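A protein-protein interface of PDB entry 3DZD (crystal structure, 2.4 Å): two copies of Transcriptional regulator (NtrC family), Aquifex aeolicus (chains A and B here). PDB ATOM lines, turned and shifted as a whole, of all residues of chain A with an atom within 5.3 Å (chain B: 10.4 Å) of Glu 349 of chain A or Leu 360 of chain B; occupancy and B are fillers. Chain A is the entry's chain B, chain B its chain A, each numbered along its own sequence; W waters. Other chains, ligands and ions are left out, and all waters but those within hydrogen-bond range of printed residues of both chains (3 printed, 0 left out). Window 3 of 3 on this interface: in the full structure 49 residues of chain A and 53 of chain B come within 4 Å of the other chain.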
ATOM      1  N   TRP A 343     -27.576   9.438 -24.310  1.00  0.00           N
ATOM      2  CA  TRP A 343     -26.744  10.452 -23.671  1.00  0.00           C
ATOM      3  C   TRP A 343     -27.235  11.862 -23.953  1.00  0.00           C
ATOM      4  O   TRP A 343     -26.502  12.664 -24.521  1.00  0.00           O
ATOM      5  CB  TRP A 343     -25.277  10.326 -24.088  1.00  0.00           C
ATOM      6  CG  TRP A 343     -24.697   8.949 -23.930  1.00  0.00           C
ATOM      7  CD1 TRP A 343     -24.335   8.092 -24.928  1.00  0.00           C
ATOM      8  CD2 TRP A 343     -24.407   8.272 -22.700  1.00  0.00           C
ATOM      9  NE1 TRP A 343     -23.838   6.930 -24.399  1.00  0.00           N
ATOM     10  CE2 TRP A 343     -23.877   7.008 -23.033  1.00  0.00           C
ATOM     11  CE3 TRP A 343     -24.550   8.606 -21.350  1.00  0.00           C
ATOM     12  CZ2 TRP A 343     -23.489   6.083 -22.070  1.00  0.00           C
ATOM     13  CZ3 TRP A 343     -24.166   7.676 -20.390  1.00  0.00           C
ATOM     14  CH2 TRP A 343     -23.639   6.434 -20.759  1.00  0.00           C
ATOM     15  N   LYS A 344     -28.462  12.169 -23.540  1.00  0.00           N
ATOM     16  CA  LYS A 344     -28.987  13.536 -23.648  1.00  0.00           C
ATOM     17  C   LYS A 344     -28.134  14.566 -22.900  1.00  0.00           C
ATOM     18  O   LYS A 344     -28.099  15.736 -23.266  1.00  0.00           O
ATOM     19  CB  LYS A 344     -30.424  13.608 -23.130  1.00  0.00           C
ATOM     20  CG  LYS A 344     -31.448  12.876 -23.976  1.00  0.00           C
ATOM     21  CD  LYS A 344     -32.772  12.729 -23.210  1.00  0.00           C
ATOM     22  CE  LYS A 344     -33.776  11.871 -23.970  1.00  0.00           C
ATOM     23  NZ  LYS A 344     -35.096  11.819 -23.276  1.00  0.00           N
ATOM     24  N   GLY A 345     -27.469  14.141 -21.832  1.00  0.00           N
ATOM     25  CA  GLY A 345     -26.576  15.026 -21.104  1.00  0.00           C
ATOM     26  C   GLY A 345     -25.150  14.906 -21.614  1.00  0.00           C
ATOM     27  O   GLY A 345     -24.224  15.464 -21.042  1.00  0.00           O
ATOM     28  N   ASN A 346     -24.977  14.126 -22.672  1.00  0.00           N
ATOM     29  CA  ASN A 346     -23.693  13.989 -23.332  1.00  0.00           C
ATOM     30  C   ASN A 346     -22.502  13.602 -22.453  1.00  0.00           C
ATOM     31  O   ASN A 346     -22.608  12.662 -21.677  1.00  0.00           O
ATOM     32  CB  ASN A 346     -23.435  15.225 -24.190  1.00  0.00           C
ATOM     33  CG  ASN A 346     -24.313  15.230 -25.440  1.00  0.00           C
ATOM     34  OD1 ASN A 346     -24.145  14.388 -26.307  1.00  0.00           O
ATOM     35  ND2 ASN A 346     -25.280  16.135 -25.499  1.00  0.00           N
ATOM     36  N   VAL A 347     -21.366  14.284 -22.598  1.00  0.00           N
ATOM     37  CA  VAL A 347     -20.167  13.896 -21.859  1.00  0.00           C
ATOM     38  C   VAL A 347     -20.343  14.155 -20.358  1.00  0.00           C
ATOM     39  O   VAL A 347     -19.822  13.418 -19.524  1.00  0.00           O
ATOM     40  CB  VAL A 347     -18.884  14.634 -22.373  1.00  0.00           C
ATOM     41  CG1 VAL A 347     -17.637  14.207 -21.575  1.00  0.00           C
ATOM     42  CG2 VAL A 347     -18.684  14.417 -23.884  1.00  0.00           C
ATOM     43  N   ARG A 348     -21.072  15.214 -20.021  1.00  0.00           N
ATOM     44  CA  ARG A 348     -21.382  15.522 -18.628  1.00  0.00           C
ATOM     45  C   ARG A 348     -22.131  14.343 -18.002  1.00  0.00           C
ATOM     46  O   ARG A 348     -21.815  13.905 -16.900  1.00  0.00           O
ATOM     47  CB  ARG A 348     -22.238  16.784 -18.567  1.00  0.00           C
ATOM     48  CG  ARG A 348     -22.196  17.571 -17.264  1.00  0.00           C
ATOM     49  CD  ARG A 348     -22.533  19.047 -17.539  1.00  0.00           C
ATOM     50  NE  ARG A 348     -23.909  19.208 -18.014  1.00  0.00           N
ATOM     51  CZ  ARG A 348     -24.349  20.257 -18.709  1.00  0.00           C
ATOM     52  NH1 ARG A 348     -23.520  21.248 -19.027  1.00  0.00           N
ATOM     53  NH2 ARG A 348     -25.622  20.311 -19.091  1.00  0.00           N
ATOM     54  N   GLU A 349     -23.119  13.816 -18.717  1.00  0.00           N
ATOM     55  CA  GLU A 349     -23.883  12.671 -18.223  1.00  0.00           C
ATOM     56  C   GLU A 349     -23.004  11.427 -18.063  1.00  0.00           C
ATOM     57  O   GLU A 349     -23.081  10.733 -17.049  1.00  0.00           O
ATOM     58  CB  GLU A 349     -25.079  12.373 -19.136  1.00  0.00           C
ATOM     59  CG  GLU A 349     -26.053  11.364 -18.555  1.00  0.00           C
ATOM     60  CD  GLU A 349     -27.121  10.929 -19.543  1.00  0.00           C
ATOM     61  OE1 GLU A 349     -27.265  11.530 -20.635  1.00  0.00           O
ATOM     62  OE2 GLU A 349     -27.824   9.959 -19.236  1.00  0.00           O
ATOM     63  N   LEU A 350     -22.165  11.156 -19.063  1.00  0.00           N
ATOM     64  CA  LEU A 350     -21.274  10.001 -19.024  1.00  0.00           C
ATOM     65  C   LEU A 350     -20.309  10.079 -17.844  1.00  0.00           C
ATOM     66  O   LEU A 350     -20.149   9.110 -17.093  1.00  0.00           O
ATOM     67  CB  LEU A 350     -20.454   9.900 -20.302  1.00  0.00           C
ATOM     68  CG  LEU A 350     -19.449   8.743 -20.265  1.00  0.00           C
ATOM     69  CD1 LEU A 350     -20.161   7.370 -20.283  1.00  0.00           C
ATOM     70  CD2 LEU A 350     -18.478   8.851 -21.408  1.00  0.00           C
ATOM     71  N   LYS A 351     -19.661  11.231 -17.703  1.00  0.00           N
ATOM     72  CA  LYS A 351     -18.649  11.418 -16.686  1.00  0.00           C
ATOM     73  C   LYS A 351     -19.227  11.139 -15.299  1.00  0.00           C
ATOM     74  O   LYS A 351     -18.675  10.354 -14.527  1.00  0.00           O
ATOM     75  CB  LYS A 351     -18.114  12.839 -16.753  1.00  0.00           C
ATOM     76  CG  LYS A 351     -17.255  13.243 -15.608  1.00  0.00           C
ATOM     77  CD  LYS A 351     -17.228  14.751 -15.506  1.00  0.00           C
ATOM     78  CE  LYS A 351     -16.923  15.205 -14.092  1.00  0.00           C
ATOM     79  NZ  LYS A 351     -17.440  16.578 -13.828  1.00  0.00           N
ATOM     80  N   ASN A 352     -20.352  11.777 -15.009  1.00  0.00           N
ATOM     81  CA  ASN A 352     -21.026  11.601 -13.744  1.00  0.00           C
ATOM     82  C   ASN A 352     -21.460  10.152 -13.501  1.00  0.00           C
ATOM     83  O   ASN A 352     -21.394   9.657 -12.372  1.00  0.00           O
ATOM     84  CB  ASN A 352     -22.214  12.547 -13.663  1.00  0.00           C
ATOM     85  CG  ASN A 352     -23.101  12.256 -12.492  1.00  0.00           C
ATOM     86  OD1 ASN A 352     -24.014  11.438 -12.580  1.00  0.00           O
ATOM     87  ND2 ASN A 352     -22.855  12.938 -11.387  1.00  0.00           N
ATOM     88  N   LEU A 353     -21.901   9.479 -14.564  1.00  0.00           N
ATOM     89  CA  LEU A 353     -22.317   8.082 -14.467  1.00  0.00           C
ATOM     90  C   LEU A 353     -21.126   7.202 -14.095  1.00  0.00           C
ATOM     91  O   LEU A 353     -21.250   6.276 -13.308  1.00  0.00           O
ATOM     92  CB  LEU A 353     -22.928   7.594 -15.780  1.00  0.00           C
ATOM     93  CG  LEU A 353     -23.293   6.108 -15.799  1.00  0.00           C
ATOM     94  CD1 LEU A 353     -24.307   5.818 -14.710  1.00  0.00           C
ATOM     95  CD2 LEU A 353     -23.828   5.652 -17.153  1.00  0.00           C
ATOM     96  N   ILE A 354     -19.960   7.490 -14.650  1.00  0.00           N
ATOM     97  CA  ILE A 354     -18.810   6.647 -14.371  1.00  0.00           C
ATOM     98  C   ILE A 354     -18.244   6.939 -12.987  1.00  0.00           C
ATOM     99  O   ILE A 354     -17.720   6.049 -12.323  1.00  0.00           O
ATOM    100  CB  ILE A 354     -17.717   6.805 -15.424  1.00  0.00           C
ATOM    101  CG1 ILE A 354     -18.255   6.390 -16.790  1.00  0.00           C
ATOM    102  CG2 ILE A 354     -16.495   5.978 -15.045  1.00  0.00           C
ATOM    103  CD1 ILE A 354     -18.496   4.911 -16.927  1.00  0.00           C
ATOM    104  N   LEU B 316     -27.948  20.990  -5.296  1.00  0.00           N
ATOM    105  CA  LEU B 316     -29.114  21.031  -6.167  1.00  0.00           C
ATOM    106  C   LEU B 316     -29.252  22.402  -6.824  1.00  0.00           C
ATOM    107  O   LEU B 316     -29.558  22.494  -8.007  1.00  0.00           O
ATOM    108  CB  LEU B 316     -30.377  20.700  -5.374  1.00  0.00           C
ATOM    109  CG  LEU B 316     -31.690  20.731  -6.156  1.00  0.00           C
ATOM    110  CD1 LEU B 316     -31.726  19.605  -7.182  1.00  0.00           C
ATOM    111  CD2 LEU B 316     -32.879  20.643  -5.207  1.00  0.00           C
ATOM    112  N   PHE B 319     -26.118  23.120  -9.346  1.00  0.00           N
ATOM    113  CA  PHE B 319     -26.178  22.361 -10.586  1.00  0.00           C
ATOM    114  C   PHE B 319     -27.378  22.757 -11.443  1.00  0.00           C
ATOM    115  O   PHE B 319     -27.230  22.988 -12.640  1.00  0.00           O
ATOM    116  CB  PHE B 319     -26.169  20.850 -10.317  1.00  0.00           C
ATOM    117  CG  PHE B 319     -24.875  20.351  -9.756  1.00  0.00           C
ATOM    118  CD1 PHE B 319     -23.668  20.739 -10.319  1.00  0.00           C
ATOM    119  CD2 PHE B 319     -24.856  19.502  -8.653  1.00  0.00           C
ATOM    120  CE1 PHE B 319     -22.464  20.288  -9.799  1.00  0.00           C
ATOM    121  CE2 PHE B 319     -23.664  19.043  -8.130  1.00  0.00           C
ATOM    122  CZ  PHE B 319     -22.469  19.437  -8.697  1.00  0.00           C
ATOM    123  N   ALA B 320     -28.557  22.839 -10.828  1.00  0.00           N
ATOM    124  CA  ALA B 320     -29.765  23.250 -11.539  1.00  0.00           C
ATOM    125  C   ALA B 320     -29.567  24.594 -12.242  1.00  0.00           C
ATOM    126  O   ALA B 320     -30.044  24.805 -13.359  1.00  0.00           O
ATOM    127  CB  ALA B 320     -30.959  23.311 -10.587  1.00  0.00           C
ATOM    128  N   TYR B 323     -26.720  23.772 -15.095  1.00  0.00           N
ATOM    129  CA  TYR B 323     -27.150  22.920 -16.204  1.00  0.00           C
ATOM    130  C   TYR B 323     -28.535  23.337 -16.709  1.00  0.00           C
ATOM    131  O   TYR B 323     -29.299  22.516 -17.233  1.00  0.00           O
ATOM    132  CB  TYR B 323     -27.170  21.437 -15.792  1.00  0.00           C
ATOM    133  CG  TYR B 323     -25.862  20.918 -15.230  1.00  0.00           C
ATOM    134  CD1 TYR B 323     -24.675  21.599 -15.450  1.00  0.00           C
ATOM    135  CD2 TYR B 323     -25.814  19.726 -14.511  1.00  0.00           C
ATOM    136  CE1 TYR B 323     -23.477  21.135 -14.948  1.00  0.00           C
ATOM    137  CE2 TYR B 323     -24.611  19.244 -13.999  1.00  0.00           C
ATOM    138  CZ  TYR B 323     -23.446  19.961 -14.217  1.00  0.00           C
ATOM    139  OH  TYR B 323     -22.239  19.507 -13.730  1.00  0.00           O
ATOM    140  N   LYS B 324     -28.857  24.615 -16.527  1.00  0.00           N
ATOM    141  CA  LYS B 324     -30.146  25.162 -16.935  1.00  0.00           C
ATOM    142  C   LYS B 324     -31.318  24.217 -16.673  1.00  0.00           C
ATOM    143  O   LYS B 324     -32.096  23.946 -17.579  1.00  0.00           O
ATOM    144  CB  LYS B 324     -30.122  25.537 -18.423  1.00  0.00           C
ATOM    145  CG  LYS B 324     -28.917  26.378 -18.854  1.00  0.00           C
ATOM    146  CD  LYS B 324     -28.884  26.586 -20.364  1.00  0.00           C
ATOM    147  CE  LYS B 324     -30.200  27.177 -20.870  1.00  0.00           C
ATOM    148  NZ  LYS B 324     -30.225  27.378 -22.354  1.00  0.00           N
ATOM    149  N   LYS B 325     -31.455  23.714 -15.452  1.00  0.00           N
ATOM    150  CA  LYS B 325     -32.609  22.871 -15.138  1.00  0.00           C
ATOM    151  C   LYS B 325     -33.605  23.593 -14.231  1.00  0.00           C
ATOM    152  O   LYS B 325     -33.275  24.603 -13.611  1.00  0.00           O
ATOM    153  CB  LYS B 325     -32.184  21.527 -14.528  1.00  0.00           C
ATOM    154  CG  LYS B 325     -31.276  20.676 -15.418  1.00  0.00           C
ATOM    155  CD  LYS B 325     -31.831  20.541 -16.830  1.00  0.00           C
ATOM    156  CE  LYS B 325     -31.109  19.459 -17.621  1.00  0.00           C
ATOM    157  NZ  LYS B 325     -31.609  18.115 -17.214  1.00  0.00           N
ATOM    158  N   ASN B 326     -34.824  23.075 -14.161  1.00  0.00           N
ATOM    159  CA  ASN B 326     -35.870  23.730 -13.391  1.00  0.00           C
ATOM    160  C   ASN B 326     -36.349  22.867 -12.225  1.00  0.00           C
ATOM    161  O   ASN B 326     -37.542  22.610 -12.072  1.00  0.00           O
ATOM    162  CB  ASN B 326     -37.039  24.114 -14.304  1.00  0.00           C
ATOM    163  CG  ASN B 326     -37.961  25.149 -13.678  1.00  0.00           C
ATOM    164  OD1 ASN B 326     -37.874  25.441 -12.482  1.00  0.00           O
ATOM    165  ND2 ASN B 326     -38.855  25.707 -14.489  1.00  0.00           N
ATOM    166  N   CYS B 327     -35.400  22.424 -11.407  1.00  0.00           N
ATOM    167  CA  CYS B 327     -35.696  21.598 -10.243  1.00  0.00           C
ATOM    168  C   CYS B 327     -34.950  22.144  -9.038  1.00  0.00           C
ATOM    169  O   CYS B 327     -33.803  21.773  -8.783  1.00  0.00           O
ATOM    170  CB  CYS B 327     -35.273  20.153 -10.498  1.00  0.00           C
ATOM    171  SG  CYS B 327     -33.568  19.991 -11.087  1.00  0.00           S
ATOM    172  N   ASN B 352     -22.055  13.891  -6.183  1.00  0.00           N
ATOM    173  CA  ASN B 352     -22.238  13.163  -7.407  1.00  0.00           C
ATOM    174  C   ASN B 352     -23.656  12.629  -7.547  1.00  0.00           C
ATOM    175  O   ASN B 352     -24.195  12.581  -8.647  1.00  0.00           O
ATOM    176  CB  ASN B 352     -21.237  12.022  -7.489  1.00  0.00           C
ATOM    177  CG  ASN B 352     -21.586  11.037  -8.578  1.00  0.00           C
ATOM    178  OD1 ASN B 352     -22.406  10.147  -8.381  1.00  0.00           O
ATOM    179  ND2 ASN B 352     -20.967  11.198  -9.736  1.00  0.00           N
ATOM    180  N   LEU B 353     -24.263  12.237  -6.433  1.00  0.00           N
ATOM    181  CA  LEU B 353     -25.632  11.741  -6.464  1.00  0.00           C
ATOM    182  C   LEU B 353     -26.638  12.844  -6.816  1.00  0.00           C
ATOM    183  O   LEU B 353     -27.637  12.589  -7.477  1.00  0.00           O
ATOM    184  CB  LEU B 353     -26.006  11.068  -5.135  1.00  0.00           C
ATOM    185  CG  LEU B 353     -27.477  10.670  -5.028  1.00  0.00           C
ATOM    186  CD1 LEU B 353     -27.642   9.238  -4.554  1.00  0.00           C
ATOM    187  CD2 LEU B 353     -28.239  11.615  -4.116  1.00  0.00           C
ATOM    188  N   ILE B 354     -26.370  14.067  -6.377  1.00  0.00           N
ATOM    189  CA  ILE B 354     -27.283  15.179  -6.620  1.00  0.00           C
ATOM    190  C   ILE B 354     -27.075  15.691  -8.032  1.00  0.00           C
ATOM    191  O   ILE B 354     -28.012  16.169  -8.670  1.00  0.00           O
ATOM    192  CB  ILE B 354     -27.045  16.353  -5.642  1.00  0.00           C
ATOM    193  CG1 ILE B 354     -27.378  15.945  -4.204  1.00  0.00           C
ATOM    194  CG2 ILE B 354     -27.880  17.555  -6.029  1.00  0.00           C
ATOM    195  CD1 ILE B 354     -28.831  15.582  -3.990  1.00  0.00           C
ATOM    196  N   GLU B 355     -25.842  15.592  -8.516  1.00  0.00           N
ATOM    197  CA  GLU B 355     -25.523  16.101  -9.839  1.00  0.00           C
ATOM    198  C   GLU B 355     -26.208  15.208 -10.847  1.00  0.00           C
ATOM    199  O   GLU B 355     -26.689  15.663 -11.888  1.00  0.00           O
ATOM    200  CB  GLU B 355     -24.020  16.095 -10.090  1.00  0.00           C
ATOM    201  CG  GLU B 355     -23.652  16.793 -11.388  1.00  0.00           C
ATOM    202  CD  GLU B 355     -22.287  16.401 -11.922  1.00  0.00           C
ATOM    203  OE1 GLU B 355     -21.689  15.438 -11.410  1.00  0.00           O
ATOM    204  OE2 GLU B 355     -21.810  17.055 -12.871  1.00  0.00           O
ATOM    205  N   ARG B 356     -26.238  13.926 -10.510  1.00  0.00           N
ATOM    206  CA  ARG B 356     -26.906  12.930 -11.319  1.00  0.00           C
ATOM    207  C   ARG B 356     -28.383  13.285 -11.399  1.00  0.00           C
ATOM    208  O   ARG B 356     -28.947  13.399 -12.481  1.00  0.00           O
ATOM    209  CB  ARG B 356     -26.718  11.554 -10.689  1.00  0.00           C
ATOM    210  CG  ARG B 356     -27.594  10.472 -11.262  1.00  0.00           C
ATOM    211  CD  ARG B 356     -26.933   9.775 -12.430  1.00  0.00           C
ATOM    212  NE  ARG B 356     -27.698   8.584 -12.806  1.00  0.00           N
ATOM    213  CZ  ARG B 356     -27.716   8.050 -14.024  1.00  0.00           C
ATOM    214  NH1 ARG B 356     -27.013   8.595 -15.012  1.00  0.00           N
ATOM    215  NH2 ARG B 356     -28.452   6.972 -14.250  1.00  0.00           N
ATOM    216  N   ALA B 357     -28.996  13.482 -10.239  1.00  0.00           N
ATOM    217  CA  ALA B 357     -30.404  13.838 -10.164  1.00  0.00           C
ATOM    218  C   ALA B 357     -30.767  14.990 -11.104  1.00  0.00           C
ATOM    219  O   ALA B 357     -31.799  14.952 -11.757  1.00  0.00           O
ATOM    220  CB  ALA B 357     -30.773  14.186  -8.734  1.00  0.00           C
ATOM    221  N   VAL B 358     -29.908  16.004 -11.157  1.00  0.00           N
ATOM    222  CA  VAL B 358     -30.153  17.212 -11.928  1.00  0.00           C
ATOM    223  C   VAL B 358     -29.971  16.975 -13.424  1.00  0.00           C
ATOM    224  O   VAL B 358     -30.690  17.542 -14.250  1.00  0.00           O
ATOM    225  CB  VAL B 358     -29.209  18.350 -11.482  1.00  0.00           C
ATOM    226  CG1 VAL B 358     -29.411  19.592 -12.344  1.00  0.00           C
ATOM    227  CG2 VAL B 358     -29.432  18.681 -10.011  1.00  0.00           C
ATOM    228  N   ILE B 359     -28.995  16.140 -13.765  1.00  0.00           N
ATOM    229  CA  ILE B 359     -28.727  15.788 -15.154  1.00  0.00           C
ATOM    230  C   ILE B 359     -29.939  15.099 -15.800  1.00  0.00           C
ATOM    231  O   ILE B 359     -30.236  15.316 -16.971  1.00  0.00           O
ATOM    232  CB  ILE B 359     -27.444  14.927 -15.266  1.00  0.00           C
ATOM    233  CG1 ILE B 359     -26.205  15.829 -15.182  1.00  0.00           C
ATOM    234  CG2 ILE B 359     -27.445  14.127 -16.554  1.00  0.00           C
ATOM    235  CD1 ILE B 359     -24.890  15.100 -14.903  1.00  0.00           C
ATOM    236  N   LEU B 360     -30.645  14.295 -15.012  1.00  0.00           N
ATOM    237  CA  LEU B 360     -31.874  13.638 -15.441  1.00  0.00           C
ATOM    238  C   LEU B 360     -33.102  14.374 -14.915  1.00  0.00           C
ATOM    239  O   LEU B 360     -34.102  13.748 -14.575  1.00  0.00           O
ATOM    240  CB  LEU B 360     -31.906  12.218 -14.864  1.00  0.00           C
ATOM    241  CG  LEU B 360     -30.569  11.470 -14.876  1.00  0.00           C
ATOM    242  CD1 LEU B 360     -30.693  10.061 -14.254  1.00  0.00           C
ATOM    243  CD2 LEU B 360     -30.018  11.403 -16.306  1.00  0.00           C
ATOM    244  N   CYS B 361     -33.037  15.693 -14.842  1.00  0.00           N
ATOM    245  CA  CYS B 361     -34.003  16.440 -14.044  1.00  0.00           C
ATOM    246  C   CYS B 361     -35.445  16.472 -14.551  1.00  0.00           C
ATOM    247  O   CYS B 361     -35.735  16.084 -15.680  1.00  0.00           O
ATOM    248  CB  CYS B 361     -33.517  17.870 -13.848  1.00  0.00           C
ATOM    249  SG  CYS B 361     -34.291  18.676 -12.452  1.00  0.00           S
ATOM    250  N   GLU B 362     -36.337  16.944 -13.681  1.00  0.00           N
ATOM    251  CA  GLU B 362     -37.728  17.233 -14.022  1.00  0.00           C
ATOM    252  C   GLU B 362     -38.116  18.613 -13.489  1.00  0.00           C
ATOM    253  O   GLU B 362     -37.375  19.581 -13.654  1.00  0.00           O
ATOM    254  CB  GLU B 362     -38.666  16.181 -13.427  1.00  0.00           C
ATOM    255  CG  GLU B 362     -38.632  14.831 -14.120  1.00  0.00           C
ATOM    256  CD  GLU B 362     -39.742  13.912 -13.640  1.00  0.00           C
ATOM    257  OE1 GLU B 362     -40.491  14.311 -12.722  1.00  0.00           O
ATOM    258  OE2 GLU B 362     -39.867  12.792 -14.181  1.00  0.00           O
ATOM    259  N   GLY B 363     -39.277  18.693 -12.844  1.00  0.00           N
ATOM    260  CA  GLY B 363     -39.714  19.918 -12.194  1.00  0.00           C
ATOM    261  C   GLY B 363     -39.252  20.004 -10.748  1.00  0.00           C
ATOM    262  O   GLY B 363     -38.821  21.060 -10.285  1.00  0.00           O
ATOM    263  N   GLU B 364     -39.356  18.888 -10.029  1.00  0.00           N
ATOM    264  CA  GLU B 364     -38.879  18.797  -8.649  1.00  0.00           C
ATOM    265  C   GLU B 364     -38.321  17.402  -8.386  1.00  0.00           C
ATOM    266  O   GLU B 364     -38.837  16.414  -8.908  1.00  0.00           O
ATOM    267  CB  GLU B 364     -39.998  19.113  -7.656  1.00  0.00           C
ATOM    268  CG  GLU B 364     -40.482  20.559  -7.682  1.00  0.00           C
ATOM    269  CD  GLU B 364     -41.625  20.792  -8.661  1.00  0.00           C
ATOM    270  OE1 GLU B 364     -41.779  19.998  -9.613  1.00  0.00           O
ATOM    271  OE2 GLU B 364     -42.373  21.776  -8.475  1.00  0.00           O
ATOM    272  N   VAL B 365     -37.274  17.321  -7.571  1.00  0.00           N
ATOM    273  CA  VAL B 365     -36.544  16.063  -7.403  1.00  0.00           C
ATOM    274  C   VAL B 365     -37.082  15.157  -6.291  1.00  0.00           C
ATOM    275  O   VAL B 365     -37.184  15.556  -5.131  1.00  0.00           O
ATOM    276  CB  VAL B 365     -35.012  16.290  -7.233  1.00  0.00           C
ATOM    277  CG1 VAL B 365     -34.379  16.673  -8.563  1.00  0.00           C
ATOM    278  CG2 VAL B 365     -34.736  17.352  -6.189  1.00  0.00           C
ATOM    279  N   ILE B 366     -37.432  13.934  -6.680  1.00  0.00           N
ATOM    280  CA  ILE B 366     -37.856  12.898  -5.747  1.00  0.00           C
ATOM    281  C   ILE B 366     -36.839  11.758  -5.815  1.00  0.00           C
ATOM    282  O   ILE B 366     -35.895  11.819  -6.604  1.00  0.00           O
ATOM    283  CB  ILE B 366     -39.283  12.405  -6.049  1.00  0.00           C
ATOM    284  CG1 ILE B 366     -40.174  13.592  -6.435  1.00  0.00           C
ATOM    285  CG2 ILE B 366     -39.856  11.667  -4.844  1.00  0.00           C
ATOM    286  CD1 ILE B 366     -41.560  13.212  -6.920  1.00  0.00           C
ATOM    287  N   PRO B 368     -35.570   8.117  -6.349  1.00  0.00           N
ATOM    288  CA  PRO B 368     -35.245   6.726  -6.685  1.00  0.00           C
ATOM    289  C   PRO B 368     -33.854   6.334  -6.172  1.00  0.00           C
ATOM    290  O   PRO B 368     -33.722   5.810  -5.060  1.00  0.00           O
ATOM    291  CB  PRO B 368     -35.272   6.722  -8.219  1.00  0.00           C
ATOM    292  CG  PRO B 368     -36.116   7.900  -8.588  1.00  0.00           C
ATOM    293  CD  PRO B 368     -35.811   8.931  -7.551  1.00  0.00           C
HETATM  294  O   HOH W   1     -25.143  10.744 -14.930  1.00  0.00           O
HETATM  295  O   HOH W   2     -27.659  22.315 -19.367  1.00  0.00           O
HETATM  296  O   HOH W   3     -27.037   7.604 -18.060  1.00  0.00           O
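ND2 of Asn 352 of chain A sits close to ND2 of Asn 352 of chain B (3.1 Å). OE1 of Glu 355 of chain B sits at hydrogen-bond distance from ND2 of Asn 352 of chain A (2.8 Å).
The side-chain sulfur of Cys 327 of chain B forms a disulfide with the side-chain sulfur of Cys 361 of chain B, at 2.0 Å. The side-chain amino group (NZ) of Lys 325 of chain B sits at hydrogen-bond distance from the backbone carbonyl oxygen (O) of Ile 359 of chain B, at 3.1 Å. The side-chain carboxylate of Glu 349 of chain A is in hydrogen-bond range of the backbone NH of Lys 344 of chain A (3.2 Å). OH of Tyr 323 of chain B is in hydrogen-bond range of OE2 of Glu 355 of chain B (2.6 Å). The backbone NH of Gly 345 of chain A lies within hydrogen-bond range of the side-chain carboxylate of Glu 349 of chain A, at 2.9 Å.
CE1 of Tyr 323 of chain B touches CD of Arg 348 of chain A, 3.5 Å away. Arg 348 of chain A touches Ile 359 of chain B (O to CD1, 3.9 Å). Ile 359 of chain B touches Glu 349 of chain A. Leu 360 of chain B touches Glu 349 of chain A (CD2 to OE2, 3.9 Å). OD1 of Asn 352 of chain A touches CB of Arg 356 of chain B (3.3 Å). Asn 352 of chain A touches Ile 359 of chain B (CB to CD1, 3.9 Å). CD1 of Leu 353 of chain A touches NH1 of Arg 356 of chain B, at 3.9 Å.
Glu 349 of chain A touches two residues of chain B. Of chain A, only Glu 349 comes within 4 Å of Leu 360 of chain B. Asn 352 of chain A touches just these residues of chain B: Asn 352, Glu 355, Arg 356 and Ile 359. Leu 353 of chain A touches just one residue of chain B: Arg 356 (3.9 Å). Printed residues of chain A within 4 Å of Tyr 323 of chain B: Arg 348. Of the printed residues of chain A, Ile 359 of chain B touches Arg 348, Glu 349 and Asn 352. Of the printed residues of chain A, Arg 356 of chain B touches Asn 352 (3.3 Å) and Leu 353 (3.9 Å). Cys 327 of chain B touches none of the printed residues of chain A. Asn 326 of chain B touches none of the printed residues of chain A. The nearest residue of chain B that does not touch Glu 349 of chain A is Arg 356 of chain B (4.5 Å). The nearest printed residue of chain A that does not touch Leu 360 of chain B is Gly 345 of chain A (6.7 Å).
Of the 12 printed residues of chain A, 4 touch a printed residue of chain B. Of the 24 printed residues of chain B, 6 touch a printed residue of chain A. Among the printed residues, 9 pairs touch across the chains.
Asn 352 of chain A touches its own counterpart, Asn 352 of chain B. Of the 9 pairs that touch across the chains among the printed residues, 1 has its exchanged pair printed and touching as well.
Water W1 lies within hydrogen-bond range of OD1 of Asn 352 of chain A (2.7 Å), NH1 of Arg 356 of chain B (2.8 Å), O of Glu 349 of chain A (3.0 Å) and N of Leu 353 of chain A (3.5 Å). Water W2 lies within hydrogen-bond range of the backbone carbonyl oxygen of Tyr 323 of chain B (2.7 Å) and the guanidinium group of Arg 348 of chain A (2.9 Å). Water W3 bridges OE2 of Glu 349 of chain A (2.7 Å) and NH1 of Arg 356 of chain B (3.2 Å).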
